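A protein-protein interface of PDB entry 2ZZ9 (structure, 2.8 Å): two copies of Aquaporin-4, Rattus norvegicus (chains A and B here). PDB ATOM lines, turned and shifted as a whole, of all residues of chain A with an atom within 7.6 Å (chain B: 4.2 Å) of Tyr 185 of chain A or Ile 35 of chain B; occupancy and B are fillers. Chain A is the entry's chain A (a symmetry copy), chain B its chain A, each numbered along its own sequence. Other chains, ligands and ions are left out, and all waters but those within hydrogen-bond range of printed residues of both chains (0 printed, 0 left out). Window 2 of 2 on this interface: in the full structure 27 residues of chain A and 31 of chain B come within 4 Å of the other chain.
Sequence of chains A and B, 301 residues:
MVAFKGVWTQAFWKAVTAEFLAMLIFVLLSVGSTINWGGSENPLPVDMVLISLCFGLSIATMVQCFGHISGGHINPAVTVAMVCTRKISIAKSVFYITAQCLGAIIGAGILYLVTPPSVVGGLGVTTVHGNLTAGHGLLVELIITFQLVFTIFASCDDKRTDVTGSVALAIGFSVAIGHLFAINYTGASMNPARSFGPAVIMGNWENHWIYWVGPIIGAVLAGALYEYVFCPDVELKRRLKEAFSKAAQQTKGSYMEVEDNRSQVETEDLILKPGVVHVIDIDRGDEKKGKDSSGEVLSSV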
ATOM      1  N   THR A 127      18.724 -25.890   4.859  1.00  0.00           N
ATOM      2  CA  THR A 127      18.809 -26.862   3.776  1.00  0.00           C
ATOM      3  C   THR A 127      20.180 -26.693   3.087  1.00  0.00           C
ATOM      4  O   THR A 127      20.541 -25.601   2.649  1.00  0.00           O
ATOM      5  CB  THR A 127      17.512 -26.795   2.829  1.00  0.00           C
ATOM      6  OG1 THR A 127      16.978 -28.109   2.619  1.00  0.00           O
ATOM      7  CG2 THR A 127      17.755 -26.095   1.493  1.00  0.00           C
ATOM      8  N   VAL A 128      20.950 -27.774   3.043  1.00  0.00           N
ATOM      9  CA  VAL A 128      22.349 -27.727   2.615  1.00  0.00           C
ATOM     10  C   VAL A 128      22.488 -27.622   1.109  1.00  0.00           C
ATOM     11  O   VAL A 128      22.337 -28.628   0.409  1.00  0.00           O
ATOM     12  CB  VAL A 128      23.148 -29.013   3.074  1.00  0.00           C
ATOM     13  CG1 VAL A 128      24.631 -28.941   2.665  1.00  0.00           C
ATOM     14  CG2 VAL A 128      23.017 -29.245   4.580  1.00  0.00           C
ATOM     15  N   HIS A 129      22.784 -26.425   0.606  1.00  0.00           N
ATOM     16  CA  HIS A 129      23.231 -26.304  -0.778  1.00  0.00           C
ATOM     17  C   HIS A 129      24.112 -25.120  -1.073  1.00  0.00           C
ATOM     18  O   HIS A 129      24.465 -24.336  -0.202  1.00  0.00           O
ATOM     19  CB  HIS A 129      22.062 -26.339  -1.772  1.00  0.00           C
ATOM     20  CG  HIS A 129      22.489 -26.596  -3.189  1.00  0.00           C
ATOM     21  ND1 HIS A 129      22.994 -27.811  -3.603  1.00  0.00           N
ATOM     22  CD2 HIS A 129      22.512 -25.786  -4.276  1.00  0.00           C
ATOM     23  CE1 HIS A 129      23.301 -27.742  -4.888  1.00  0.00           C
ATOM     24  NE2 HIS A 129      23.023 -26.522  -5.317  1.00  0.00           N
ATOM     25  N   GLY A 130      24.402 -24.992  -2.354  1.00  0.00           N
ATOM     26  CA  GLY A 130      25.504 -24.226  -2.894  1.00  0.00           C
ATOM     27  C   GLY A 130      26.177 -25.217  -3.839  1.00  0.00           C
ATOM     28  O   GLY A 130      27.130 -24.878  -4.531  1.00  0.00           O
ATOM     29  N   ASN A 131      25.643 -26.445  -3.858  1.00  0.00           N
ATOM     30  CA  ASN A 131      26.073 -27.555  -4.718  1.00  0.00           C
ATOM     31  C   ASN A 131      26.903 -28.498  -3.915  1.00  0.00           C
ATOM     32  O   ASN A 131      27.345 -29.531  -4.412  1.00  0.00           O
ATOM     33  CB  ASN A 131      26.805 -27.087  -5.981  1.00  0.00           C
ATOM     34  CG  ASN A 131      25.845 -26.500  -7.031  1.00  0.00           C
ATOM     35  OD1 ASN A 131      24.962 -27.200  -7.531  1.00  0.00           O
ATOM     36  ND2 ASN A 131      26.018 -25.214  -7.361  1.00  0.00           N
ATOM     37  N   LEU A 132      27.070 -28.139  -2.646  1.00  0.00           N
ATOM     38  CA  LEU A 132      27.919 -28.845  -1.693  1.00  0.00           C
ATOM     39  C   LEU A 132      27.437 -30.260  -1.493  1.00  0.00           C
ATOM     40  O   LEU A 132      26.281 -30.566  -1.783  1.00  0.00           O
ATOM     41  CB  LEU A 132      27.869 -28.140  -0.339  1.00  0.00           C
ATOM     42  CG  LEU A 132      27.574 -26.639  -0.328  1.00  0.00           C
ATOM     43  CD1 LEU A 132      26.908 -26.245   0.965  1.00  0.00           C
ATOM     44  CD2 LEU A 132      28.832 -25.864  -0.532  1.00  0.00           C
ATOM     45  N   THR A 133      28.318 -31.126  -0.993  1.00  0.00           N
ATOM     46  CA  THR A 133      27.897 -32.485  -0.624  1.00  0.00           C
ATOM     47  C   THR A 133      27.189 -32.459   0.723  1.00  0.00           C
ATOM     48  O   THR A 133      26.676 -31.426   1.155  1.00  0.00           O
ATOM     49  CB  THR A 133      29.078 -33.507  -0.547  1.00  0.00           C
ATOM     50  OG1 THR A 133      29.952 -33.155   0.534  1.00  0.00           O
ATOM     51  CG2 THR A 133      29.857 -33.580  -1.866  1.00  0.00           C
ATOM     52  N   HIS A 136      30.442 -31.713   3.296  1.00  0.00           N
ATOM     53  CA  HIS A 136      30.749 -30.296   3.316  1.00  0.00           C
ATOM     54  C   HIS A 136      29.809 -29.612   4.276  1.00  0.00           C
ATOM     55  O   HIS A 136      30.238 -28.866   5.154  1.00  0.00           O
ATOM     56  CB  HIS A 136      30.527 -29.713   1.931  1.00  0.00           C
ATOM     57  CG  HIS A 136      31.548 -30.142   0.935  1.00  0.00           C
ATOM     58  ND1 HIS A 136      31.258 -30.301  -0.402  1.00  0.00           N
ATOM     59  CD2 HIS A 136      32.862 -30.450   1.082  1.00  0.00           C
ATOM     60  CE1 HIS A 136      32.352 -30.685  -1.037  1.00  0.00           C
ATOM     61  NE2 HIS A 136      33.338 -30.783  -0.160  1.00  0.00           N
ATOM     62  N   GLY A 137      28.516 -29.885   4.077  1.00  0.00           N
ATOM     63  CA  GLY A 137      27.446 -29.349   4.900  1.00  0.00           C
ATOM     64  C   GLY A 137      27.576 -29.843   6.320  1.00  0.00           C
ATOM     65  O   GLY A 137      27.254 -29.125   7.255  1.00  0.00           O
ATOM     66  N   VAL A 140      30.783 -27.580   7.421  1.00  0.00           N
ATOM     67  CA  VAL A 140      30.447 -26.167   7.608  1.00  0.00           C
ATOM     68  C   VAL A 140      29.681 -26.006   8.915  1.00  0.00           C
ATOM     69  O   VAL A 140      29.971 -25.086   9.682  1.00  0.00           O
ATOM     70  CB  VAL A 140      29.629 -25.597   6.442  1.00  0.00           C
ATOM     71  CG1 VAL A 140      29.622 -24.083   6.474  1.00  0.00           C
ATOM     72  CG2 VAL A 140      30.201 -26.067   5.138  1.00  0.00           C
ATOM     73  N   GLU A 141      28.729 -26.913   9.168  1.00  0.00           N
ATOM     74  CA  GLU A 141      28.035 -26.994  10.476  1.00  0.00           C
ATOM     75  C   GLU A 141      28.965 -27.400  11.617  1.00  0.00           C
ATOM     76  O   GLU A 141      29.089 -26.676  12.601  1.00  0.00           O
ATOM     77  CB  GLU A 141      26.815 -27.933  10.445  1.00  0.00           C
ATOM     78  CG  GLU A 141      25.577 -27.399   9.692  1.00  0.00           C
ATOM     79  CD  GLU A 141      25.005 -26.115  10.259  1.00  0.00           C
ATOM     80  OE1 GLU A 141      25.760 -25.328  10.859  1.00  0.00           O
ATOM     81  OE2 GLU A 141      23.792 -25.877  10.074  1.00  0.00           O
ATOM     82  N   HIS A 179      26.132 -17.033  11.404  1.00  0.00           N
ATOM     83  CA  HIS A 179      25.164 -16.798  10.333  1.00  0.00           C
ATOM     84  C   HIS A 179      25.793 -15.938   9.250  1.00  0.00           C
ATOM     85  O   HIS A 179      25.639 -16.213   8.061  1.00  0.00           O
ATOM     86  CB  HIS A 179      23.933 -16.099  10.890  1.00  0.00           C
ATOM     87  CG  HIS A 179      22.998 -17.025  11.590  1.00  0.00           C
ATOM     88  ND1 HIS A 179      23.136 -17.356  12.921  1.00  0.00           N
ATOM     89  CD2 HIS A 179      21.928 -17.717  11.136  1.00  0.00           C
ATOM     90  CE1 HIS A 179      22.186 -18.208  13.260  1.00  0.00           C
ATOM     91  NE2 HIS A 179      21.439 -18.443  12.196  1.00  0.00           N
ATOM     92  N   PHE A 181      28.249 -16.013   7.776  1.00  0.00           N
ATOM     93  CA  PHE A 181      29.055 -16.761   6.791  1.00  0.00           C
ATOM     94  C   PHE A 181      28.275 -17.933   6.167  1.00  0.00           C
ATOM     95  O   PHE A 181      28.248 -18.094   4.941  1.00  0.00           O
ATOM     96  CB  PHE A 181      30.389 -17.250   7.404  1.00  0.00           C
ATOM     97  CG  PHE A 181      30.935 -18.518   6.777  1.00  0.00           C
ATOM     98  CD1 PHE A 181      31.490 -18.511   5.501  1.00  0.00           C
ATOM     99  CD2 PHE A 181      30.902 -19.731   7.471  1.00  0.00           C
ATOM    100  CE1 PHE A 181      32.005 -19.694   4.929  1.00  0.00           C
ATOM    101  CE2 PHE A 181      31.405 -20.923   6.890  1.00  0.00           C
ATOM    102  CZ  PHE A 181      31.954 -20.897   5.617  1.00  0.00           C
ATOM    103  N   ALA A 182      27.644 -18.730   7.023  1.00  0.00           N
ATOM    104  CA  ALA A 182      27.213 -20.065   6.652  1.00  0.00           C
ATOM    105  C   ALA A 182      25.865 -20.052   5.986  1.00  0.00           C
ATOM    106  O   ALA A 182      25.464 -21.058   5.385  1.00  0.00           O
ATOM    107  CB  ALA A 182      27.217 -21.023   7.910  1.00  0.00           C
ATOM    108  N   ILE A 183      25.173 -18.913   6.082  1.00  0.00           N
ATOM    109  CA  ILE A 183      23.758 -18.823   5.637  1.00  0.00           C
ATOM    110  C   ILE A 183      23.493 -19.459   4.254  1.00  0.00           C
ATOM    111  O   ILE A 183      22.611 -20.335   4.149  1.00  0.00           O
ATOM    112  CB  ILE A 183      23.112 -17.398   5.812  1.00  0.00           C
ATOM    113  CG1 ILE A 183      22.889 -17.087   7.294  1.00  0.00           C
ATOM    114  CG2 ILE A 183      21.767 -17.318   5.115  1.00  0.00           C
ATOM    115  CD1 ILE A 183      22.344 -15.710   7.583  1.00  0.00           C
ATOM    116  N   ASN A 184      24.256 -19.074   3.225  1.00  0.00           N
ATOM    117  CA  ASN A 184      24.062 -19.703   1.915  1.00  0.00           C
ATOM    118  C   ASN A 184      24.664 -21.099   1.813  1.00  0.00           C
ATOM    119  O   ASN A 184      24.192 -21.921   1.030  1.00  0.00           O
ATOM    120  CB  ASN A 184      24.569 -18.828   0.762  1.00  0.00           C
ATOM    121  CG  ASN A 184      23.843 -17.505   0.665  1.00  0.00           C
ATOM    122  OD1 ASN A 184      24.410 -16.501   0.223  1.00  0.00           O
ATOM    123  ND2 ASN A 184      22.588 -17.489   1.105  1.00  0.00           N
ATOM    124  N   TYR A 185      25.705 -21.369   2.596  1.00  0.00           N
ATOM    125  CA  TYR A 185      26.273 -22.717   2.671  1.00  0.00           C
ATOM    126  C   TYR A 185      25.268 -23.771   3.185  1.00  0.00           C
ATOM    127  O   TYR A 185      24.977 -24.760   2.506  1.00  0.00           O
ATOM    128  CB  TYR A 185      27.500 -22.735   3.579  1.00  0.00           C
ATOM    129  CG  TYR A 185      28.733 -22.084   3.004  1.00  0.00           C
ATOM    130  CD1 TYR A 185      29.710 -22.851   2.351  1.00  0.00           C
ATOM    131  CD2 TYR A 185      28.942 -20.705   3.134  1.00  0.00           C
ATOM    132  CE1 TYR A 185      30.852 -22.251   1.816  1.00  0.00           C
ATOM    133  CE2 TYR A 185      30.060 -20.095   2.595  1.00  0.00           C
ATOM    134  CZ  TYR A 185      31.018 -20.872   1.944  1.00  0.00           C
ATOM    135  OH  TYR A 185      32.139 -20.268   1.433  1.00  0.00           O
ATOM    136  N   THR A 186      24.734 -23.563   4.379  1.00  0.00           N
ATOM    137  CA  THR A 186      24.140 -24.683   5.078  1.00  0.00           C
ATOM    138  C   THR A 186      22.779 -24.358   5.640  1.00  0.00           C
ATOM    139  O   THR A 186      22.044 -25.250   6.074  1.00  0.00           O
ATOM    140  CB  THR A 186      25.077 -25.174   6.252  1.00  0.00           C
ATOM    141  OG1 THR A 186      25.020 -26.597   6.374  1.00  0.00           O
ATOM    142  CG2 THR A 186      24.665 -24.543   7.584  1.00  0.00           C
ATOM    143  N   GLY A 187      22.445 -23.079   5.639  1.00  0.00           N
ATOM    144  CA  GLY A 187      21.304 -22.603   6.417  1.00  0.00           C
ATOM    145  C   GLY A 187      21.789 -21.852   7.642  1.00  0.00           C
ATOM    146  O   GLY A 187      21.054 -21.048   8.218  1.00  0.00           O
ATOM    147  N   ALA A 188      23.045 -22.110   8.004  1.00  0.00           N
ATOM    148  CA  ALA A 188      23.642 -21.668   9.261  1.00  0.00           C
ATOM    149  C   ALA A 188      22.829 -22.069  10.504  1.00  0.00           C
ATOM    150  O   ALA A 188      22.466 -21.190  11.293  1.00  0.00           O
ATOM    151  CB  ALA A 188      23.889 -20.155   9.225  1.00  0.00           C
ATOM    152  N   TYR A 211      21.969 -31.947  10.457  1.00  0.00           N
ATOM    153  CA  TYR A 211      21.810 -30.857  11.421  1.00  0.00           C
ATOM    154  C   TYR A 211      21.750 -31.357  12.859  1.00  0.00           C
ATOM    155  O   TYR A 211      21.511 -30.580  13.786  1.00  0.00           O
ATOM    156  CB  TYR A 211      20.556 -30.033  11.088  1.00  0.00           C
ATOM    157  CG  TYR A 211      20.679 -29.326   9.771  1.00  0.00           C
ATOM    158  CD1 TYR A 211      21.478 -28.192   9.644  1.00  0.00           C
ATOM    159  CD2 TYR A 211      20.023 -29.805   8.639  1.00  0.00           C
ATOM    160  CE1 TYR A 211      21.615 -27.527   8.424  1.00  0.00           C
ATOM    161  CE2 TYR A 211      20.152 -29.149   7.400  1.00  0.00           C
ATOM    162  CZ  TYR A 211      20.951 -28.006   7.303  1.00  0.00           C
ATOM    163  OH  TYR A 211      21.096 -27.354   6.098  1.00  0.00           O
ATOM    164  N   VAL B  31      36.733 -14.243   6.092  1.00  0.00           N
ATOM    165  CA  VAL B  31      37.107 -14.249   4.677  1.00  0.00           C
ATOM    166  C   VAL B  31      35.994 -14.946   3.883  1.00  0.00           C
ATOM    167  O   VAL B  31      35.672 -14.556   2.762  1.00  0.00           O
ATOM    168  CB  VAL B  31      38.513 -14.865   4.441  1.00  0.00           C
ATOM    169  CG1 VAL B  31      38.587 -15.620   3.144  1.00  0.00           C
ATOM    170  CG2 VAL B  31      39.556 -13.779   4.463  1.00  0.00           C
ATOM    171  N   GLY B  32      35.387 -15.948   4.507  1.00  0.00           N
ATOM    172  CA  GLY B  32      34.249 -16.622   3.941  1.00  0.00           C
ATOM    173  C   GLY B  32      33.048 -15.713   3.813  1.00  0.00           C
ATOM    174  O   GLY B  32      32.023 -16.113   3.261  1.00  0.00           O
ATOM    175  N   SER B  33      33.142 -14.495   4.331  1.00  0.00           N
ATOM    176  CA  SER B  33      32.019 -13.581   4.195  1.00  0.00           C
ATOM    177  C   SER B  33      32.164 -12.734   2.950  1.00  0.00           C
ATOM    178  O   SER B  33      31.170 -12.271   2.372  1.00  0.00           O
ATOM    179  CB  SER B  33      31.872 -12.694   5.393  1.00  0.00           C
ATOM    180  OG  SER B  33      30.531 -12.303   5.467  1.00  0.00           O
ATOM    181  N   THR B  34      33.411 -12.548   2.536  1.00  0.00           N
ATOM    182  CA  THR B  34      33.712 -11.774   1.356  1.00  0.00           C
ATOM    183  C   THR B  34      33.102 -12.469   0.128  1.00  0.00           C
ATOM    184  O   THR B  34      32.894 -11.845  -0.919  1.00  0.00           O
ATOM    185  CB  THR B  34      35.234 -11.578   1.190  1.00  0.00           C
ATOM    186  OG1 THR B  34      35.830 -12.758   0.633  1.00  0.00           O
ATOM    187  CG2 THR B  34      35.892 -11.259   2.544  1.00  0.00           C
ATOM    188  N   ILE B  35      32.798 -13.758   0.290  1.00  0.00           N
ATOM    189  CA  ILE B  35      32.170 -14.571  -0.750  1.00  0.00           C
ATOM    190  C   ILE B  35      30.926 -13.885  -1.334  1.00  0.00           C
ATOM    191  O   ILE B  35      30.086 -13.380  -0.604  1.00  0.00           O
ATOM    192  CB  ILE B  35      31.888 -16.021  -0.238  1.00  0.00           C
ATOM    193  CG1 ILE B  35      33.190 -16.695   0.209  1.00  0.00           C
ATOM    194  CG2 ILE B  35      31.253 -16.867  -1.313  1.00  0.00           C
ATOM    195  CD1 ILE B  35      34.263 -16.788  -0.875  1.00  0.00           C
ATOM    196  N   ASN B  36      30.844 -13.854  -2.658  1.00  0.00           N
ATOM    197  CA  ASN B  36      29.809 -13.107  -3.366  1.00  0.00           C
ATOM    198  C   ASN B  36      28.867 -14.019  -4.144  1.00  0.00           C
ATOM    199  O   ASN B  36      29.222 -14.481  -5.231  1.00  0.00           O
ATOM    200  CB  ASN B  36      30.475 -12.124  -4.330  1.00  0.00           C
ATOM    201  CG  ASN B  36      29.529 -11.062  -4.821  1.00  0.00           C
ATOM    202  OD1 ASN B  36      29.676  -9.891  -4.486  1.00  0.00           O
ATOM    203  ND2 ASN B  36      28.538 -11.463  -5.603  1.00  0.00           N
ATOM    204  N   TRP B  37      27.669 -14.263  -3.611  1.00  0.00           N
ATOM    205  CA  TRP B  37      26.780 -15.266  -4.207  1.00  0.00           C
ATOM    206  C   TRP B  37      26.095 -14.781  -5.477  1.00  0.00           C
ATOM    207  O   TRP B  37      24.898 -14.492  -5.516  1.00  0.00           O
ATOM    208  CB  TRP B  37      25.811 -15.839  -3.182  1.00  0.00           C
ATOM    209  CG  TRP B  37      26.527 -16.669  -2.168  1.00  0.00           C
ATOM    210  CD1 TRP B  37      26.771 -18.019  -2.225  1.00  0.00           C
ATOM    211  CD2 TRP B  37      27.124 -16.205  -0.952  1.00  0.00           C
ATOM    212  NE1 TRP B  37      27.472 -18.422  -1.109  1.00  0.00           N
ATOM    213  CE2 TRP B  37      27.700 -17.328  -0.313  1.00  0.00           C
ATOM    214  CE3 TRP B  37      27.223 -14.948  -0.336  1.00  0.00           C
ATOM    215  CZ2 TRP B  37      28.371 -17.228   0.915  1.00  0.00           C
ATOM    216  CZ3 TRP B  37      27.885 -14.848   0.891  1.00  0.00           C
ATOM    217  CH2 TRP B  37      28.454 -15.981   1.500  1.00  0.00           C
ATOM    218  N   LEU B 111      38.447 -23.443   3.669  1.00  0.00           N
ATOM    219  CA  LEU B 111      37.367 -22.652   3.084  1.00  0.00           C
ATOM    220  C   LEU B 111      37.176 -22.957   1.618  1.00  0.00           C
ATOM    221  O   LEU B 111      36.047 -23.117   1.163  1.00  0.00           O
ATOM    222  CB  LEU B 111      37.593 -21.157   3.268  1.00  0.00           C
ATOM    223  CG  LEU B 111      36.498 -20.325   2.600  1.00  0.00           C
ATOM    224  CD1 LEU B 111      35.165 -20.447   3.325  1.00  0.00           C
ATOM    225  CD2 LEU B 111      36.891 -18.867   2.464  1.00  0.00           C
ATOM    226  N   VAL B 114      34.909 -25.819   0.616  1.00  0.00           N
ATOM    227  CA  VAL B 114      33.621 -25.887   1.274  1.00  0.00           C
ATOM    228  C   VAL B 114      32.744 -24.841   0.607  1.00  0.00           C
ATOM    229  O   VAL B 114      31.529 -25.003   0.486  1.00  0.00           O
ATOM    230  CB  VAL B 114      33.764 -25.689   2.817  1.00  0.00           C
ATOM    231  CG1 VAL B 114      32.620 -24.899   3.417  1.00  0.00           C
ATOM    232  CG2 VAL B 114      33.898 -27.032   3.500  1.00  0.00           C
ATOM    233  N   THR B 115      33.376 -23.758   0.174  1.00  0.00           N
ATOM    234  CA  THR B 115      32.710 -22.844  -0.721  1.00  0.00           C
ATOM    235  C   THR B 115      32.652 -23.520  -2.068  1.00  0.00           C
ATOM    236  O   THR B 115      33.582 -24.224  -2.444  1.00  0.00           O
ATOM    237  CB  THR B 115      33.405 -21.511  -0.823  1.00  0.00           C
ATOM    238  OG1 THR B 115      32.730 -20.708  -1.799  1.00  0.00           O
ATOM    239  CG2 THR B 115      34.843 -21.704  -1.209  1.00  0.00           C
ATOM    240  N   PRO B 116      31.527 -23.362  -2.767  1.00  0.00           N
ATOM    241  CA  PRO B 116      31.257 -23.927  -4.074  1.00  0.00           C
ATOM    242  C   PRO B 116      32.113 -23.320  -5.213  1.00  0.00           C
ATOM    243  O   PRO B 116      33.317 -23.134  -5.035  1.00  0.00           O
ATOM    244  CB  PRO B 116      29.770 -23.620  -4.255  1.00  0.00           C
ATOM    245  CG  PRO B 116      29.254 -23.349  -2.887  1.00  0.00           C
ATOM    246  CD  PRO B 116      30.355 -22.635  -2.254  1.00  0.00           C
ATOM    247  N   SER B 118      31.615 -20.221  -6.638  1.00  0.00           N
ATOM    248  CA  SER B 118      31.269 -18.803  -6.651  1.00  0.00           C
ATOM    249  C   SER B 118      32.388 -18.020  -5.987  1.00  0.00           C
ATOM    250  O   SER B 118      32.270 -16.807  -5.795  1.00  0.00           O
ATOM    251  CB  SER B 118      29.962 -18.563  -5.890  1.00  0.00           C
ATOM    252  OG  SER B 118      30.179 -18.547  -4.483  1.00  0.00           O
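Gly 130 of chain A touches Pro 116 of chain B (O to CB, 2.9 Å). Pro 116 of chain B touches Leu 132 of chain A (CG to CD2, 3.5 Å). Val 140 of chain A touches Val 114 of chain B. CD1 of Phe 181 of chain A touches O of Gly 32 of chain B, 3.3 Å away. Phe 181 of chain A touches Leu 111 of chain B. Trp 37 of chain B touches Asn 184 of chain A (CD2 to OD1, 3.0 Å). Ile 35 of chain B touches Tyr 185 of chain A (CG1 to OH, 3.9 Å). CE2 of Tyr 185 of chain A touches CZ2 of Trp 37 of chain B (3.7 Å). CD1 of Leu 111 of chain B touches OH of Tyr 185 of chain A (3.6 Å). Tyr 185 of chain A touches Val 114 of chain B (CE1 to O, 3.1 Å).
Of the printed residues of chain B, Gly 130 of chain A touches Pro 116 (2.9 Å). Of the printed residues of chain B, Phe 181 of chain A touches Gly 32 (3.3 Å) and Leu 111 (3.6 Å). Of the printed residues of chain B, Asn 184 of chain A touches Trp 37. Tyr 185 of chain A touches just these residues of chain B: Ile 35, Trp 37, Leu 111, Val 114 and Thr 115. Thr 186 of chain A touches none of the printed residues of chain B. Printed residues of chain A within 4 Å of Gly 32 of chain B: Phe 181 (3.3 Å). Thr 34 of chain B touches none of the printed residues of chain A. Of the printed residues of chain A, Pro 116 of chain B touches Gly 130 (2.9 Å) and Leu 132 (3.5 Å). The nearest residue of chain B that does not touch Tyr 185 of chain A is Pro 116 of chain B (4.1 Å). The nearest residue of chain A that does not touch Ile 35 of chain B is Phe 181 of chain A (5.7 Å).
Printed residues of chain B that touch a printed residue of chain A: Gly 32, Ile 35, Trp 37, Leu 111, Val 114, Thr 115 and Pro 116. Printed residues of chain A that touch a printed residue of chain B: Gly 130, Leu 132, Val 140, Phe 181, Asn 184 and Tyr 185. Among the printed residues, 12 pairs touch across the chains. Among the printed residues, no Asp or Glu carboxylate lies within 4 Å of a Lys or Arg side-chain nitrogen of the other chain.
No position is printed for both chains.
The side-chain hydroxyl of Tyr 185 of chain A sits close to the side-chain hydroxyl of Thr 115 of chain B (3.3 Å).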
